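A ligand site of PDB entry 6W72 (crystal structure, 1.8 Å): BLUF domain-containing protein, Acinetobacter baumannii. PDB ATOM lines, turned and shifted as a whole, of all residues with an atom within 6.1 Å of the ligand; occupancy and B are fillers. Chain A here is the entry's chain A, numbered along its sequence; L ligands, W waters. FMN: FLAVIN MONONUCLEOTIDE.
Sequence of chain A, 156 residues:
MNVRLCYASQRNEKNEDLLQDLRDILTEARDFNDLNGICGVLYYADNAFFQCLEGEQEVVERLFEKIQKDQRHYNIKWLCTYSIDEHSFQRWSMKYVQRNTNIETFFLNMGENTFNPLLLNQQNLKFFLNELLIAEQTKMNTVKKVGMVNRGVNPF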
ATOM      1  N   TYR A   7      20.915  -6.086   8.402  1.00  0.00           N
ATOM      2  CA  TYR A   7      19.781  -6.443   7.510  1.00  0.00           C
ATOM      3  C   TYR A   7      20.328  -6.758   6.121  1.00  0.00           C
ATOM      4  O   TYR A   7      21.434  -6.316   5.749  1.00  0.00           O
ATOM      5  CB  TYR A   7      18.705  -5.329   7.456  1.00  0.00           C
ATOM      6  CG  TYR A   7      19.158  -4.109   6.702  1.00  0.00           C
ATOM      7  CD1 TYR A   7      18.955  -4.003   5.341  1.00  0.00           C
ATOM      8  CD2 TYR A   7      19.888  -3.106   7.322  1.00  0.00           C
ATOM      9  CE1 TYR A   7      19.422  -2.906   4.629  1.00  0.00           C
ATOM     10  CE2 TYR A   7      20.350  -2.003   6.633  1.00  0.00           C
ATOM     11  CZ  TYR A   7      20.112  -1.911   5.268  1.00  0.00           C
ATOM     12  OH  TYR A   7      20.617  -0.886   4.550  1.00  0.00           O
ATOM     13  N   SER A   9      18.781  -6.625   1.902  1.00  0.00           N
ATOM     14  CA  SER A   9      17.728  -6.060   1.031  1.00  0.00           C
ATOM     15  C   SER A   9      18.056  -6.339  -0.427  1.00  0.00           C
ATOM     16  O   SER A   9      19.164  -6.854  -0.697  1.00  0.00           O
ATOM     17  CB  SER A   9      17.593  -4.590   1.333  1.00  0.00           C
ATOM     18  OG  SER A   9      18.705  -3.883   0.811  1.00  0.00           O
ATOM     19  N   ILE A  25      24.266   6.691  -2.132  1.00  0.00           N
ATOM     20  CA  ILE A  25      24.055   6.006  -0.826  1.00  0.00           C
ATOM     21  C   ILE A  25      25.279   6.213   0.095  1.00  0.00           C
ATOM     22  O   ILE A  25      25.113   6.617   1.244  1.00  0.00           O
ATOM     23  CB  ILE A  25      23.729   4.518  -1.028  1.00  0.00           C
ATOM     24  CG1 ILE A  25      22.372   4.346  -1.713  1.00  0.00           C
ATOM     25  CG2 ILE A  25      23.818   3.746   0.259  1.00  0.00           C
ATOM     26  CD1 ILE A  25      22.221   3.041  -2.420  1.00  0.00           C
ATOM     27  N   GLU A  28      25.737  10.012   1.212  1.00  0.00           N
ATOM     28  CA  GLU A  28      24.700  10.318   2.224  1.00  0.00           C
ATOM     29  C   GLU A  28      25.050   9.601   3.534  1.00  0.00           C
ATOM     30  O   GLU A  28      25.019  10.223   4.626  1.00  0.00           O
ATOM     31  CB  GLU A  28      23.335   9.843   1.722  1.00  0.00           C
ATOM     32  CG  GLU A  28      22.837  10.548   0.466  1.00  0.00           C
ATOM     33  CD  GLU A  28      21.647   9.872  -0.203  1.00  0.00           C
ATOM     34  OE1 GLU A  28      20.878   9.246   0.522  1.00  0.00           O
ATOM     35  OE2 GLU A  28      21.469  10.021  -1.447  1.00  0.00           O
ATOM     36  N   ALA A  29      25.333   8.308   3.455  1.00  0.00           N
ATOM     37  CA  ALA A  29      25.619   7.462   4.637  1.00  0.00           C
ATOM     38  C   ALA A  29      26.838   7.995   5.401  1.00  0.00           C
ATOM     39  O   ALA A  29      26.760   8.070   6.645  1.00  0.00           O
ATOM     40  CB  ALA A  29      25.782   6.020   4.212  1.00  0.00           C
ATOM     41  N   ARG A  30      27.942   8.291   4.711  1.00  0.00           N
ATOM     42  CA  ARG A  30      29.215   8.715   5.349  1.00  0.00           C
ATOM     43  C   ARG A  30      29.014  10.078   6.035  1.00  0.00           C
ATOM     44  O   ARG A  30      29.437  10.221   7.180  1.00  0.00           O
ATOM     45  CB  ARG A  30      30.343   8.638   4.321  1.00  0.00           C
ATOM     46  CG  ARG A  30      30.763   7.206   4.022  1.00  0.00           C
ATOM     47  CD  ARG A  30      31.591   7.077   2.769  1.00  0.00           C
ATOM     48  NE  ARG A  30      31.920   5.676   2.578  1.00  0.00           N
ATOM     49  CZ  ARG A  30      32.531   5.161   1.518  1.00  0.00           C
ATOM     50  NH1 ARG A  30      32.831   5.942   0.490  1.00  0.00           N
ATOM     51  NH2 ARG A  30      32.753   3.865   1.445  1.00  0.00           N
ATOM     52  N   PHE A  32      25.983  11.540   7.195  1.00  0.00           N
ATOM     53  CA  PHE A  32      25.057  11.385   8.350  1.00  0.00           C
ATOM     54  C   PHE A  32      25.709  10.567   9.467  1.00  0.00           C
ATOM     55  O   PHE A  32      25.564  10.951  10.640  1.00  0.00           O
ATOM     56  CB  PHE A  32      23.753  10.733   7.921  1.00  0.00           C
ATOM     57  CG  PHE A  32      22.744  10.605   9.040  1.00  0.00           C
ATOM     58  CD1 PHE A  32      21.881  11.647   9.338  1.00  0.00           C
ATOM     59  CD2 PHE A  32      22.700   9.462   9.822  1.00  0.00           C
ATOM     60  CE1 PHE A  32      20.960  11.518  10.352  1.00  0.00           C
ATOM     61  CE2 PHE A  32      21.794   9.342  10.864  1.00  0.00           C
ATOM     62  CZ  PHE A  32      20.902  10.372  11.115  1.00  0.00           C
ATOM     63  N   ASN A  33      26.350   9.455   9.147  1.00  0.00           N
ATOM     64  CA  ASN A  33      26.903   8.487  10.137  1.00  0.00           C
ATOM     65  C   ASN A  33      28.003   9.169  10.948  1.00  0.00           C
ATOM     66  O   ASN A  33      28.020   9.019  12.148  1.00  0.00           O
ATOM     67  CB  ASN A  33      27.365   7.195   9.461  1.00  0.00           C
ATOM     68  CG  ASN A  33      26.201   6.345   8.978  1.00  0.00           C
ATOM     69  OD1 ASN A  33      25.054   6.746   9.062  1.00  0.00           O
ATOM     70  ND2 ASN A  33      26.487   5.156   8.443  1.00  0.00           N
ATOM     71  N   ILE A  38      27.662   6.878  14.071  1.00  0.00           N
ATOM     72  CA  ILE A  38      27.388   5.528  13.490  1.00  0.00           C
ATOM     73  C   ILE A  38      28.572   5.138  12.607  1.00  0.00           C
ATOM     74  O   ILE A  38      29.184   6.020  11.960  1.00  0.00           O
ATOM     75  CB  ILE A  38      26.058   5.510  12.726  1.00  0.00           C
ATOM     76  CG1 ILE A  38      24.902   5.822  13.690  1.00  0.00           C
ATOM     77  CG2 ILE A  38      25.848   4.173  12.009  1.00  0.00           C
ATOM     78  CD1 ILE A  38      23.716   6.339  13.017  1.00  0.00           C
ATOM     79  N   LEU A  42      28.677  -1.636   4.389  1.00  0.00           N
ATOM     80  CA  LEU A  42      27.699  -1.900   3.323  1.00  0.00           C
ATOM     81  C   LEU A  42      28.372  -2.821   2.295  1.00  0.00           C
ATOM     82  O   LEU A  42      29.389  -2.425   1.657  1.00  0.00           O
ATOM     83  CB  LEU A  42      27.262  -0.596   2.699  1.00  0.00           C
ATOM     84  CG  LEU A  42      26.223  -0.757   1.581  1.00  0.00           C
ATOM     85  CD1 LEU A  42      24.935  -1.331   2.140  1.00  0.00           C
ATOM     86  CD2 LEU A  42      25.924   0.536   0.859  1.00  0.00           C
ATOM     87  N   PHE A  49      21.891  -5.929  -1.072  1.00  0.00           N
ATOM     88  CA  PHE A  49      22.660  -5.199  -0.057  1.00  0.00           C
ATOM     89  C   PHE A  49      22.716  -6.036   1.227  1.00  0.00           C
ATOM     90  O   PHE A  49      21.714  -6.687   1.591  1.00  0.00           O
ATOM     91  CB  PHE A  49      21.975  -3.867   0.244  1.00  0.00           C
ATOM     92  CG  PHE A  49      22.044  -2.873  -0.874  1.00  0.00           C
ATOM     93  CD1 PHE A  49      23.210  -2.191  -1.141  1.00  0.00           C
ATOM     94  CD2 PHE A  49      20.909  -2.611  -1.646  1.00  0.00           C
ATOM     95  CE1 PHE A  49      23.237  -1.242  -2.144  1.00  0.00           C
ATOM     96  CE2 PHE A  49      20.958  -1.694  -2.670  1.00  0.00           C
ATOM     97  CZ  PHE A  49      22.113  -0.991  -2.897  1.00  0.00           C
ATOM     98  N   GLN A  51      23.894  -4.770   5.162  1.00  0.00           N
ATOM     99  CA  GLN A  51      24.472  -3.664   5.942  1.00  0.00           C
ATOM    100  C   GLN A  51      24.493  -4.020   7.428  1.00  0.00           C
ATOM    101  O   GLN A  51      23.499  -4.623   7.990  1.00  0.00           O
ATOM    102  CB  GLN A  51      23.708  -2.360   5.747  1.00  0.00           C
ATOM    103  CG  GLN A  51      24.487  -1.144   6.221  1.00  0.00           C
ATOM    104  CD  GLN A  51      23.808   0.168   5.901  1.00  0.00           C
ATOM    105  OE1 GLN A  51      22.602   0.296   5.919  1.00  0.00           O
ATOM    106  NE2 GLN A  51      24.609   1.143   5.505  1.00  0.00           N
ATOM    107  N   LEU A  53      25.091  -1.770  10.936  1.00  0.00           N
ATOM    108  CA  LEU A  53      25.176  -0.463  11.608  1.00  0.00           C
ATOM    109  C   LEU A  53      25.582  -0.661  13.062  1.00  0.00           C
ATOM    110  O   LEU A  53      25.011  -1.502  13.730  1.00  0.00           O
ATOM    111  CB  LEU A  53      23.807   0.190  11.541  1.00  0.00           C
ATOM    112  CG  LEU A  53      23.235   0.437  10.149  1.00  0.00           C
ATOM    113  CD1 LEU A  53      21.807   0.940  10.288  1.00  0.00           C
ATOM    114  CD2 LEU A  53      24.089   1.441   9.384  1.00  0.00           C
ATOM    115  N   LEU A  63      17.821   5.210  12.376  1.00  0.00           N
ATOM    116  CA  LEU A  63      18.420   5.266  11.015  1.00  0.00           C
ATOM    117  C   LEU A  63      17.865   4.094  10.189  1.00  0.00           C
ATOM    118  O   LEU A  63      17.571   4.282   9.013  1.00  0.00           O
ATOM    119  CB  LEU A  63      19.949   5.280  11.115  1.00  0.00           C
ATOM    120  CG  LEU A  63      20.654   4.994   9.788  1.00  0.00           C
ATOM    121  CD1 LEU A  63      20.319   6.034   8.727  1.00  0.00           C
ATOM    122  CD2 LEU A  63      22.149   4.878   9.964  1.00  0.00           C
ATOM    123  N   LYS A  66      14.551   4.903   8.737  1.00  0.00           N
ATOM    124  CA  LYS A  66      14.700   5.797   7.584  1.00  0.00           C
ATOM    125  C   LYS A  66      15.128   4.986   6.356  1.00  0.00           C
ATOM    126  O   LYS A  66      14.603   5.207   5.250  1.00  0.00           O
ATOM    127  CB  LYS A  66      15.743   6.853   7.962  1.00  0.00           C
ATOM    128  CG  LYS A  66      15.925   7.974   6.959  1.00  0.00           C
ATOM    129  CD  LYS A  66      16.839   9.058   7.472  1.00  0.00           C
ATOM    130  CE  LYS A  66      18.290   8.673   7.272  1.00  0.00           C
ATOM    131  NZ  LYS A  66      19.203   9.466   8.140  1.00  0.00           N
ATOM    132  N   ILE A  67      16.077   4.073   6.549  1.00  0.00           N
ATOM    133  CA  ILE A  67      16.625   3.256   5.449  1.00  0.00           C
ATOM    134  C   ILE A  67      15.493   2.379   4.872  1.00  0.00           C
ATOM    135  O   ILE A  67      15.436   2.221   3.643  1.00  0.00           O
ATOM    136  CB  ILE A  67      17.839   2.432   5.926  1.00  0.00           C
ATOM    137  CG1 ILE A  67      19.052   3.318   6.207  1.00  0.00           C
ATOM    138  CG2 ILE A  67      18.177   1.369   4.890  1.00  0.00           C
ATOM    139  CD1 ILE A  67      20.182   2.612   6.945  1.00  0.00           C
ATOM    140  N   GLN A  68      14.570   1.882   5.710  1.00  0.00           N
ATOM    141  CA  GLN A  68      13.458   1.061   5.201  1.00  0.00           C
ATOM    142  C   GLN A  68      12.654   1.831   4.156  1.00  0.00           C
ATOM    143  O   GLN A  68      12.058   1.191   3.293  1.00  0.00           O
ATOM    144  CB  GLN A  68      12.542   0.664   6.379  1.00  0.00           C
ATOM    145  CG  GLN A  68      13.123  -0.470   7.204  1.00  0.00           C
ATOM    146  CD  GLN A  68      12.419  -0.568   8.538  1.00  0.00           C
ATOM    147  OE1 GLN A  68      11.267  -0.178   8.671  1.00  0.00           O
ATOM    148  NE2 GLN A  68      13.136  -1.048   9.533  1.00  0.00           N
ATOM    149  N   LYS A  69      12.604   3.141   4.258  1.00  0.00           N
ATOM    150  CA  LYS A  69      11.781   4.017   3.370  1.00  0.00           C
ATOM    151  C   LYS A  69      12.504   4.312   2.056  1.00  0.00           C
ATOM    152  O   LYS A  69      11.918   4.967   1.171  1.00  0.00           O
ATOM    153  CB  LYS A  69      11.474   5.333   4.087  1.00  0.00           C
ATOM    154  CG  LYS A  69      10.653   5.213   5.354  1.00  0.00           C
ATOM    155  CD  LYS A  69      10.422   6.588   5.960  1.00  0.00           C
ATOM    156  CE  LYS A  69       9.457   6.608   7.118  1.00  0.00           C
ATOM    157  NZ  LYS A  69      10.123   6.251   8.385  1.00  0.00           N
ATOM    158  N   ASP A  70      13.757   3.909   1.929  1.00  0.00           N
ATOM    159  CA  ASP A  70      14.605   4.311   0.768  1.00  0.00           C
ATOM    160  C   ASP A  70      14.171   3.511  -0.463  1.00  0.00           C
ATOM    161  O   ASP A  70      14.191   2.268  -0.439  1.00  0.00           O
ATOM    162  CB  ASP A  70      16.090   4.142   1.083  1.00  0.00           C
ATOM    163  CG  ASP A  70      17.001   4.898   0.118  1.00  0.00           C
ATOM    164  OD1 ASP A  70      16.807   4.748  -1.143  1.00  0.00           O
ATOM    165  OD2 ASP A  70      17.874   5.659   0.615  1.00  0.00           O
ATOM    166  N   ARG A  72      15.680   2.978  -3.204  1.00  0.00           N
ATOM    167  CA  ARG A  72      16.799   2.333  -3.928  1.00  0.00           C
ATOM    168  C   ARG A  72      16.923   0.857  -3.534  1.00  0.00           C
ATOM    169  O   ARG A  72      17.805   0.157  -4.062  1.00  0.00           O
ATOM    170  CB  ARG A  72      18.069   3.142  -3.721  1.00  0.00           C
ATOM    171  CG  ARG A  72      18.018   4.486  -4.425  1.00  0.00           C
ATOM    172  CD  ARG A  72      19.134   5.433  -4.047  1.00  0.00           C
ATOM    173  NE  ARG A  72      19.052   5.896  -2.680  1.00  0.00           N
ATOM    174  CZ  ARG A  72      19.803   6.875  -2.165  1.00  0.00           C
ATOM    175  NH1 ARG A  72      20.653   7.533  -2.939  1.00  0.00           N
ATOM    176  NH2 ARG A  72      19.669   7.250  -0.908  1.00  0.00           N
ATOM    177  N   HIS A  73      16.130   0.377  -2.604  1.00  0.00           N
ATOM    178  CA  HIS A  73      16.072  -1.079  -2.356  1.00  0.00           C
ATOM    179  C   HIS A  73      14.670  -1.463  -1.904  1.00  0.00           C
ATOM    180  O   HIS A  73      13.846  -0.577  -1.636  1.00  0.00           O
ATOM    181  CB  HIS A  73      17.196  -1.467  -1.360  1.00  0.00           C
ATOM    182  CG  HIS A  73      17.093  -0.898   0.007  1.00  0.00           C
ATOM    183  ND1 HIS A  73      17.894  -1.382   1.020  1.00  0.00           N
ATOM    184  CD2 HIS A  73      16.342   0.117   0.532  1.00  0.00           C
ATOM    185  CE1 HIS A  73      17.648  -0.704   2.117  1.00  0.00           C
ATOM    186  NE2 HIS A  73      16.703   0.236   1.847  1.00  0.00           N
ATOM    187  N   SER A  93      32.810   5.402   8.774  1.00  0.00           N
ATOM    188  CA  SER A  93      31.417   5.860   8.924  1.00  0.00           C
ATOM    189  C   SER A  93      30.503   4.894   8.130  1.00  0.00           C
ATOM    190  O   SER A  93      29.474   4.509   8.671  1.00  0.00           O
ATOM    191  CB  SER A  93      31.247   7.291   8.488  1.00  0.00           C
ATOM    192  OG  SER A  93      32.069   8.136   9.301  1.00  0.00           O
ATOM    193  N   MET A  94      30.937   4.476   6.938  1.00  0.00           N
ATOM    194  CA  MET A  94      30.292   3.358   6.201  1.00  0.00           C
ATOM    195  C   MET A  94      31.286   2.755   5.203  1.00  0.00           C
ATOM    196  O   MET A  94      31.527   3.355   4.142  1.00  0.00           O
ATOM    197  CB  MET A  94      29.039   3.842   5.468  1.00  0.00           C
ATOM    198  CG  MET A  94      28.242   2.725   4.815  1.00  0.00           C
ATOM    199  SD  MET A  94      27.974   1.314   5.947  1.00  0.00           S
ATOM    200  CE  MET A  94      27.060   1.992   7.323  1.00  0.00           C
HETATM  201  N1  FMN L   1      21.824   6.759   5.152  1.00  0.00           N
HETATM  202  C2  FMN L   1      22.570   7.016   6.254  1.00  0.00           C
HETATM  203  O2  FMN L   1      22.488   8.160   6.764  1.00  0.00           O
HETATM  204  N3  FMN L   1      23.359   6.102   6.826  1.00  0.00           N
HETATM  205  C4  FMN L   1      23.476   4.879   6.302  1.00  0.00           C
HETATM  206  O4  FMN L   1      24.204   4.011   6.815  1.00  0.00           O
HETATM  207  C4A FMN L   1      22.682   4.480   5.118  1.00  0.00           C
HETATM  208  N5  FMN L   1      22.783   3.248   4.567  1.00  0.00           N
HETATM  209  C5A FMN L   1      22.004   2.952   3.494  1.00  0.00           C
HETATM  210  C6  FMN L   1      22.048   1.713   2.913  1.00  0.00           C
HETATM  211  C7  FMN L   1      21.272   1.420   1.796  1.00  0.00           C
HETATM  212  C7M FMN L   1      21.350   0.078   1.156  1.00  0.00           C
HETATM  213  C8  FMN L   1      20.390   2.463   1.200  1.00  0.00           C
HETATM  214  C8M FMN L   1      19.566   2.152  -0.020  1.00  0.00           C
HETATM  215  C9  FMN L   1      20.387   3.726   1.749  1.00  0.00           C
HETATM  216  C9A FMN L   1      21.153   4.028   2.861  1.00  0.00           C
HETATM  217  N10 FMN L   1      21.077   5.293   3.471  1.00  0.00           N
HETATM  218  C10 FMN L   1      21.875   5.563   4.560  1.00  0.00           C
HETATM  219  C1' FMN L   1      20.379   6.438   2.948  1.00  0.00           C
HETATM  220  C2' FMN L   1      19.084   6.886   3.501  1.00  0.00           C
HETATM  221  O2' FMN L   1      18.185   5.787   3.379  1.00  0.00           O
HETATM  222  C3' FMN L   1      18.759   8.128   2.669  1.00  0.00           C
HETATM  223  O3' FMN L   1      19.751   9.117   2.853  1.00  0.00           O
HETATM  224  C4' FMN L   1      17.506   8.643   3.274  1.00  0.00           C
HETATM  225  O4' FMN L   1      16.427   7.974   2.592  1.00  0.00           O
HETATM  226  C5' FMN L   1      17.364  10.159   3.131  1.00  0.00           C
HETATM  227  O5' FMN L   1      16.226  10.342   3.957  1.00  0.00           O
HETATM  228  P   FMN L   1      15.621  11.805   4.153  1.00  0.00           P
HETATM  229  O1P FMN L   1      15.043  12.151   2.803  1.00  0.00           O
HETATM  230  O2P FMN L   1      14.644  11.611   5.290  1.00  0.00           O
HETATM  231  O3P FMN L   1      16.859  12.633   4.460  1.00  0.00           O
HETATM  232  O   HOH W   1      14.398   7.181   3.617  1.00  0.00           O
HETATM  233  O   HOH W   2      21.133   9.754   5.480  1.00  0.00           O
HETATM  234  O   HOH W   3      16.825  12.773   1.224  1.00  0.00           O
HETATM  235  O   HOH W   4      16.228   8.536   0.134  1.00  0.00           O
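O3' of the ligand is in hydrogen-bond range of OE1 of Glu 28 (2.6 Å).
The side-chain carboxylate (OD2) of Asp 70 is in hydrogen-bond range of an oxygen (O2') of the ligand (2.8 Å).
N3 of the ligand lies within hydrogen-bond range of OD1 of Asn 33 (2.9 Å).
A nitrogen (N5) of the ligand is in hydrogen-bond range of the side-chain amide nitrogen of Gln 51 (2.9 Å).
The side-chain amide oxygen (OD1) of Asn 33 lies close to the backbone carbonyl oxygen (O) of Ala 29, at 3.2 Å.
The backbone NH (N) of Ile 38 lies within hydrogen-bond range of the backbone carbonyl oxygen (O) of Asn 33 (2.9 Å).
The side-chain sulfur (SD) of Met 94 sits close to the side-chain amide nitrogen (NE2) of Gln 51, at 3.4 Å.
The side-chain sulfur (SD) of Met 94 lies within hydrogen-bond range of the backbone NH (N) of Leu 42, 3.4 Å away.
NE of Arg 30 sits at hydrogen-bond distance from O of Met 94 (2.8 Å).
A ring nitrogen (NE2) of His 73 lies within hydrogen-bond range of the backbone carbonyl oxygen (O) of Ile 67, at 3.0 Å.
The backbone NH of Phe 49 lies within hydrogen-bond range of the backbone carbonyl oxygen of Ser 9, 2.9 Å away.
A ring nitrogen (ND1) of His 73 lies within hydrogen-bond range of the side-chain hydroxyl (OG) of Ser 9 (2.6 Å).
OH of Tyr 7 touches C6 of the ligand, 3.4 Å away.
CD1 of Ile 25 touches C8M of the ligand, at 3.7 Å.
CB of Ala 29 touches C4 of the ligand, 3.3 Å away.
CB of Phe 32 touches O2 of the ligand (3.1 Å).
Leu 42 touches the ligand (CD1 to C7M, 3.98 Å).
CG of Phe 49 touches C7M of the ligand, at 3.6 Å.
Leu 53 touches the ligand (CD2 to O4, 3.6 Å).
Leu 63 touches the ligand (CD1 to C2, 3.5 Å).
CD of Lys 66 touches O5' of the ligand (3.8 Å).
CD1 of Ile 67 touches N5 of the ligand, 3.6 Å away.
NH2 of Arg 72 touches C3' of the ligand (3.8 Å).
ND1 of His 73 touches C7M of the ligand (3.8 Å).
CE of Met 94 touches O4 of the ligand (3.5 Å).
The nearest printed residue that does not touch the ligand is Ser 9 (4.8 Å).
Water W1 lies within hydrogen-bond range of an oxygen (O4') of the ligand (2.4 Å) and the backbone carbonyl oxygen of Lys 66 (2.6 Å).
Water W2 lies within hydrogen-bond range of an oxygen (O2) of the ligand (2.5 Å) and the side-chain amino group (NZ) of Lys 66 (3.3 Å).
Water W4 lies within hydrogen-bond range of O4' of the ligand (2.5 Å) and OD2 of Asp 70 (3.3 Å).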
